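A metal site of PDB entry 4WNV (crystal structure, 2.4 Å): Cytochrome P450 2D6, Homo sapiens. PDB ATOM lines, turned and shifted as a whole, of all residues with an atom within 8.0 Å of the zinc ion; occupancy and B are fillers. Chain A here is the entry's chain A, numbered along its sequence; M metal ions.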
ATOM      1  N   TRP A 130     -17.622  19.089  26.898  1.00  0.00           N
ATOM      2  CA  TRP A 130     -18.819  18.556  26.251  1.00  0.00           C
ATOM      3  C   TRP A 130     -18.480  17.562  25.152  1.00  0.00           C
ATOM      4  O   TRP A 130     -19.109  16.515  25.039  1.00  0.00           O
ATOM      5  CB  TRP A 130     -19.675  19.679  25.658  1.00  0.00           C
ATOM      6  CG  TRP A 130     -20.512  20.408  26.654  1.00  0.00           C
ATOM      7  CD1 TRP A 130     -21.179  19.881  27.712  1.00  0.00           C
ATOM      8  CD2 TRP A 130     -20.761  21.813  26.676  1.00  0.00           C
ATOM      9  NE1 TRP A 130     -21.841  20.872  28.405  1.00  0.00           N
ATOM     10  CE2 TRP A 130     -21.600  22.071  27.782  1.00  0.00           C
ATOM     11  CE3 TRP A 130     -20.369  22.897  25.862  1.00  0.00           C
ATOM     12  CZ2 TRP A 130     -22.050  23.360  28.110  1.00  0.00           C
ATOM     13  CZ3 TRP A 130     -20.822  24.177  26.195  1.00  0.00           C
ATOM     14  CH2 TRP A 130     -21.649  24.401  27.291  1.00  0.00           C
ATOM     15  N   ALA A 165     -26.055  20.896  20.448  1.00  0.00           N
ATOM     16  CA  ALA A 165     -27.023  21.024  21.526  1.00  0.00           C
ATOM     17  C   ALA A 165     -26.346  21.558  22.794  1.00  0.00           C
ATOM     18  O   ALA A 165     -26.914  22.384  23.500  1.00  0.00           O
ATOM     19  CB  ALA A 165     -27.698  19.684  21.806  1.00  0.00           C
ATOM     20  N   SER A 166     -25.143  21.081  23.080  1.00  0.00           N
ATOM     21  CA  SER A 166     -24.416  21.561  24.239  1.00  0.00           C
ATOM     22  C   SER A 166     -24.038  23.029  24.080  1.00  0.00           C
ATOM     23  O   SER A 166     -24.256  23.835  24.961  1.00  0.00           O
ATOM     24  CB  SER A 166     -23.171  20.712  24.493  1.00  0.00           C
ATOM     25  OG  SER A 166     -23.543  19.370  24.760  1.00  0.00           O
ATOM     26  N   LEU A 167     -23.427  23.358  22.944  1.00  0.00           N
ATOM     27  CA  LEU A 167     -23.073  24.732  22.609  1.00  0.00           C
ATOM     28  C   LEU A 167     -24.278  25.654  22.734  1.00  0.00           C
ATOM     29  O   LEU A 167     -24.195  26.728  23.333  1.00  0.00           O
ATOM     30  CB  LEU A 167     -22.506  24.793  21.178  1.00  0.00           C
ATOM     31  CG  LEU A 167     -22.555  26.106  20.379  1.00  0.00           C
ATOM     32  CD1 LEU A 167     -21.746  27.161  21.066  1.00  0.00           C
ATOM     33  CD2 LEU A 167     -22.044  25.922  18.941  1.00  0.00           C
ATOM     34  N   THR A 168     -25.407  25.258  22.148  1.00  0.00           N
ATOM     35  CA  THR A 168     -26.541  26.152  21.999  1.00  0.00           C
ATOM     36  C   THR A 168     -27.462  26.165  23.216  1.00  0.00           C
ATOM     37  O   THR A 168     -27.836  27.228  23.683  1.00  0.00           O
ATOM     38  CB  THR A 168     -27.367  25.807  20.743  1.00  0.00           C
ATOM     39  OG1 THR A 168     -27.786  24.426  20.784  1.00  0.00           O
ATOM     40  CG2 THR A 168     -26.543  26.066  19.462  1.00  0.00           C
ATOM     41  N   CYS A 169     -27.807  24.993  23.762  1.00  0.00           N
ATOM     42  CA  CYS A 169     -28.770  24.927  24.863  1.00  0.00           C
ATOM     43  C   CYS A 169     -28.182  24.388  26.173  1.00  0.00           C
ATOM     44  O   CYS A 169     -28.899  24.252  27.154  1.00  0.00           O
ATOM     45  CB  CYS A 169     -29.964  24.081  24.448  1.00  0.00           C
ATOM     46  SG  CYS A 169     -30.820  24.624  22.932  1.00  0.00           S
ATOM     47  N   GLY A 170     -26.884  24.097  26.201  1.00  0.00           N
ATOM     48  CA  GLY A 170     -26.237  23.617  27.417  1.00  0.00           C
ATOM     49  C   GLY A 170     -26.736  22.247  27.896  1.00  0.00           C
ATOM     50  O   GLY A 170     -26.721  21.946  29.107  1.00  0.00           O
ATOM     51  N   ARG A 171     -27.180  21.406  26.967  1.00  0.00           N
ATOM     52  CA  ARG A 171     -27.562  20.065  27.319  1.00  0.00           C
ATOM     53  C   ARG A 171     -27.251  19.106  26.197  1.00  0.00           C
ATOM     54  O   ARG A 171     -27.040  19.521  25.065  1.00  0.00           O
ATOM     55  CB  ARG A 171     -29.051  19.980  27.616  1.00  0.00           C
ATOM     56  CG  ARG A 171     -29.878  20.162  26.377  1.00  0.00           C
ATOM     57  CD  ARG A 171     -31.281  19.758  26.638  1.00  0.00           C
ATOM     58  NE  ARG A 171     -31.342  18.341  26.920  1.00  0.00           N
ATOM     59  CZ  ARG A 171     -32.460  17.693  27.199  1.00  0.00           C
ATOM     60  NH1 ARG A 171     -33.618  18.350  27.246  1.00  0.00           N
ATOM     61  NH2 ARG A 171     -32.428  16.386  27.444  1.00  0.00           N
ATOM     62  N   HIS A 236     -35.765  25.900  27.354  1.00  0.00           N
ATOM     63  CA  HIS A 236     -34.482  26.389  27.824  1.00  0.00           C
ATOM     64  C   HIS A 236     -34.650  27.756  28.461  1.00  0.00           C
ATOM     65  O   HIS A 236     -33.929  28.114  29.380  1.00  0.00           O
ATOM     66  CB  HIS A 236     -33.484  26.424  26.670  1.00  0.00           C
ATOM     67  CG  HIS A 236     -32.103  26.799  27.093  1.00  0.00           C
ATOM     68  ND1 HIS A 236     -31.224  27.431  26.246  1.00  0.00           N
ATOM     69  CD2 HIS A 236     -31.441  26.637  28.261  1.00  0.00           C
ATOM     70  CE1 HIS A 236     -30.072  27.630  26.864  1.00  0.00           C
ATOM     71  NE2 HIS A 236     -30.181  27.160  28.090  1.00  0.00           N
ATOM     72  N   ARG A 237     -35.617  28.512  27.976  1.00  0.00           N
ATOM     73  CA  ARG A 237     -35.859  29.859  28.468  1.00  0.00           C
ATOM     74  C   ARG A 237     -36.384  29.855  29.902  1.00  0.00           C
ATOM     75  O   ARG A 237     -36.146  30.792  30.664  1.00  0.00           O
ATOM     76  CB  ARG A 237     -36.844  30.549  27.543  1.00  0.00           C
ATOM     77  CG  ARG A 237     -36.635  32.029  27.408  1.00  0.00           C
ATOM     78  CD  ARG A 237     -37.207  32.496  26.090  1.00  0.00           C
ATOM     79  NE  ARG A 237     -37.240  33.955  25.997  1.00  0.00           N
ATOM     80  CZ  ARG A 237     -37.326  34.606  24.845  1.00  0.00           C
ATOM     81  NH1 ARG A 237     -37.387  33.914  23.703  1.00  0.00           N
ATOM     82  NH2 ARG A 237     -37.337  35.937  24.826  1.00  0.00           N
ATOM     83  N   THR A 239     -35.492  27.592  32.213  1.00  0.00           N
ATOM     84  CA  THR A 239     -34.461  27.148  33.140  1.00  0.00           C
ATOM     85  C   THR A 239     -33.283  28.119  33.228  1.00  0.00           C
ATOM     86  O   THR A 239     -32.448  28.007  34.123  1.00  0.00           O
ATOM     87  CB  THR A 239     -33.918  25.769  32.760  1.00  0.00           C
ATOM     88  OG1 THR A 239     -33.447  25.809  31.418  1.00  0.00           O
ATOM     89  CG2 THR A 239     -34.990  24.734  32.864  1.00  0.00           C
ATOM     90  N   TRP A 240     -33.220  29.072  32.290  1.00  0.00           N
ATOM     91  CA  TRP A 240     -32.133  30.038  32.226  1.00  0.00           C
ATOM     92  C   TRP A 240     -32.035  30.844  33.524  1.00  0.00           C
ATOM     93  O   TRP A 240     -33.020  31.395  34.014  1.00  0.00           O
ATOM     94  CB  TRP A 240     -32.317  31.004  31.045  1.00  0.00           C
ATOM     95  CG  TRP A 240     -31.351  32.181  30.989  1.00  0.00           C
ATOM     96  CD1 TRP A 240     -30.010  32.175  31.275  1.00  0.00           C
ATOM     97  CD2 TRP A 240     -31.659  33.534  30.609  1.00  0.00           C
ATOM     98  NE1 TRP A 240     -29.480  33.435  31.094  1.00  0.00           N
ATOM     99  CE2 TRP A 240     -30.468  34.284  30.676  1.00  0.00           C
ATOM    100  CE3 TRP A 240     -32.833  34.179  30.205  1.00  0.00           C
ATOM    101  CZ2 TRP A 240     -30.416  35.643  30.392  1.00  0.00           C
ATOM    102  CZ3 TRP A 240     -32.786  35.547  29.912  1.00  0.00           C
ATOM    103  CH2 TRP A 240     -31.579  36.255  30.002  1.00  0.00           C
ATOM    104  N   ASP A 241     -30.817  30.901  34.062  1.00  0.00           N
ATOM    105  CA  ASP A 241     -30.556  31.698  35.242  1.00  0.00           C
ATOM    106  C   ASP A 241     -29.758  32.953  34.854  1.00  0.00           C
ATOM    107  O   ASP A 241     -28.530  32.915  34.804  1.00  0.00           O
ATOM    108  CB  ASP A 241     -29.808  30.875  36.276  1.00  0.00           C
ATOM    109  CG  ASP A 241     -29.728  31.541  37.613  1.00  0.00           C
ATOM    110  OD1 ASP A 241     -29.263  30.890  38.562  1.00  0.00           O
ATOM    111  OD2 ASP A 241     -30.149  32.715  37.723  1.00  0.00           O
ATOM    112  N   PRO A 245     -23.479  33.747  34.982  1.00  0.00           N
ATOM    113  CA  PRO A 245     -22.890  33.936  33.651  1.00  0.00           C
ATOM    114  C   PRO A 245     -23.487  32.951  32.669  1.00  0.00           C
ATOM    115  O   PRO A 245     -23.748  31.808  33.062  1.00  0.00           O
ATOM    116  CB  PRO A 245     -21.394  33.646  33.865  1.00  0.00           C
ATOM    117  CG  PRO A 245     -21.162  33.941  35.307  1.00  0.00           C
ATOM    118  CD  PRO A 245     -22.443  33.548  36.011  1.00  0.00           C
ATOM    119  N   PRO A 246     -23.738  33.394  31.426  1.00  0.00           N
ATOM    120  CA  PRO A 246     -24.264  32.529  30.363  1.00  0.00           C
ATOM    121  C   PRO A 246     -23.519  31.201  30.264  1.00  0.00           C
ATOM    122  O   PRO A 246     -22.298  31.204  30.195  1.00  0.00           O
ATOM    123  CB  PRO A 246     -24.064  33.368  29.110  1.00  0.00           C
ATOM    124  CG  PRO A 246     -24.132  34.767  29.587  1.00  0.00           C
ATOM    125  CD  PRO A 246     -23.589  34.789  30.989  1.00  0.00           C
ATOM    126  N   ARG A 247     -24.255  30.091  30.292  1.00  0.00           N
ATOM    127  CA  ARG A 247     -23.665  28.748  30.203  1.00  0.00           C
ATOM    128  C   ARG A 247     -23.423  28.351  28.762  1.00  0.00           C
ATOM    129  O   ARG A 247     -22.588  27.498  28.472  1.00  0.00           O
ATOM    130  CB  ARG A 247     -24.586  27.711  30.864  1.00  0.00           C
ATOM    131  CG  ARG A 247     -24.486  27.609  32.360  1.00  0.00           C
ATOM    132  CD  ARG A 247     -25.560  26.699  32.958  1.00  0.00           C
ATOM    133  NE  ARG A 247     -26.914  27.238  32.759  1.00  0.00           N
ATOM    134  CZ  ARG A 247     -27.874  27.259  33.683  1.00  0.00           C
ATOM    135  NH1 ARG A 247     -27.645  26.782  34.914  1.00  0.00           N
ATOM    136  NH2 ARG A 247     -29.066  27.788  33.390  1.00  0.00           N
ATOM    137  N   ASP A 248     -24.186  28.950  27.865  1.00  0.00           N
ATOM    138  CA  ASP A 248     -24.260  28.491  26.490  1.00  0.00           C
ATOM    139  C   ASP A 248     -24.652  29.653  25.587  1.00  0.00           C
ATOM    140  O   ASP A 248     -24.885  30.757  26.059  1.00  0.00           O
ATOM    141  CB  ASP A 248     -25.269  27.339  26.354  1.00  0.00           C
ATOM    142  CG  ASP A 248     -26.587  27.638  27.061  1.00  0.00           C
ATOM    143  OD1 ASP A 248     -27.295  28.552  26.626  1.00  0.00           O
ATOM    144  OD2 ASP A 248     -26.907  26.949  28.042  1.00  0.00           O
ATOM    145  N   LEU A 249     -24.740  29.386  24.291  1.00  0.00           N
ATOM    146  CA  LEU A 249     -24.847  30.452  23.318  1.00  0.00           C
ATOM    147  C   LEU A 249     -26.235  31.111  23.368  1.00  0.00           C
ATOM    148  O   LEU A 249     -26.365  32.330  23.221  1.00  0.00           O
ATOM    149  CB  LEU A 249     -24.541  29.927  21.915  1.00  0.00           C
ATOM    150  CG  LEU A 249     -24.587  30.963  20.795  1.00  0.00           C
ATOM    151  CD1 LEU A 249     -23.598  30.599  19.698  1.00  0.00           C
ATOM    152  CD2 LEU A 249     -25.988  31.085  20.222  1.00  0.00           C
ATOM    153  N   THR A 250     -27.268  30.291  23.546  1.00  0.00           N
ATOM    154  CA  THR A 250     -28.639  30.788  23.692  1.00  0.00           C
ATOM    155  C   THR A 250     -28.771  31.773  24.871  1.00  0.00           C
ATOM    156  O   THR A 250     -29.533  32.726  24.812  1.00  0.00           O
ATOM    157  CB  THR A 250     -29.635  29.602  23.870  1.00  0.00           C
ATOM    158  OG1 THR A 250     -29.731  28.876  22.634  1.00  0.00           O
ATOM    159  CG2 THR A 250     -31.011  30.071  24.279  1.00  0.00           C
ATOM    160  N   GLU A 251     -28.009  31.554  25.940  1.00  0.00           N
ATOM    161  CA  GLU A 251     -28.134  32.398  27.131  1.00  0.00           C
ATOM    162  C   GLU A 251     -27.372  33.681  26.928  1.00  0.00           C
ATOM    163  O   GLU A 251     -27.849  34.745  27.311  1.00  0.00           O
ATOM    164  CB  GLU A 251     -27.639  31.669  28.393  1.00  0.00           C
ATOM    165  CG  GLU A 251     -28.465  30.435  28.754  1.00  0.00           C
ATOM    166  CD  GLU A 251     -27.972  29.780  30.041  1.00  0.00           C
ATOM    167  OE1 GLU A 251     -27.080  30.360  30.695  1.00  0.00           O
ATOM    168  OE2 GLU A 251     -28.473  28.690  30.386  1.00  0.00           O
ATOM    169  N   ALA A 252     -26.214  33.588  26.279  1.00  0.00           N
ATOM    170  CA  ALA A 252     -25.497  34.775  25.854  1.00  0.00           C
ATOM    171  C   ALA A 252     -26.406  35.617  24.958  1.00  0.00           C
ATOM    172  O   ALA A 252     -26.507  36.826  25.140  1.00  0.00           O
ATOM    173  CB  ALA A 252     -24.183  34.412  25.137  1.00  0.00           C
ATOM    174  N   LEU A 254     -29.710  35.533  24.785  1.00  0.00           N
ATOM    175  CA  LEU A 254     -30.845  36.022  25.566  1.00  0.00           C
ATOM    176  C   LEU A 254     -30.458  37.253  26.365  1.00  0.00           C
ATOM    177  O   LEU A 254     -31.228  38.213  26.453  1.00  0.00           O
ATOM    178  CB  LEU A 254     -31.389  34.928  26.491  1.00  0.00           C
ATOM    179  CG  LEU A 254     -32.227  33.842  25.787  1.00  0.00           C
ATOM    180  CD1 LEU A 254     -32.575  32.717  26.765  1.00  0.00           C
ATOM    181  CD2 LEU A 254     -33.483  34.423  25.174  1.00  0.00           C
HETATM  182 ZN    ZN M   1     -28.613  27.199  29.150  1.00  0.00          ZN
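The side-chain carboxylate of Asp 248 lies close to the backbone NH of Gly 170.
NE of Arg 247 lies within salt-bridge range of OE1 of Glu 251, 3.7 Å away.
SG of Cys 169 sits close to OG1 of Thr 168, 3.7 Å away.
OG1 of Thr 239 is in hydrogen-bond range of O of His 236, at 3.1 Å.
O of Thr 239 lies within hydrogen-bond range of NH2 of Arg 247, at 3.5 Å.
A ring nitrogen (NE2) of His 236 lies close to the backbone carbonyl oxygen (O) of Cys 169.
Cys 169 touches the zinc ion (O to ZN, 3.6 Å).
Arg 247 touches the zinc ion.
Five residues have an atom within 4 Å of the zinc ion: Cys 169, His 236, Arg 247, Asp 248 and Glu 251.
The zinc ion is bound by NE2 of His 236 (1.9 Å), OE2 of Glu 251 (1.9 Å) and OD2 of Asp 248 (2.0 Å).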
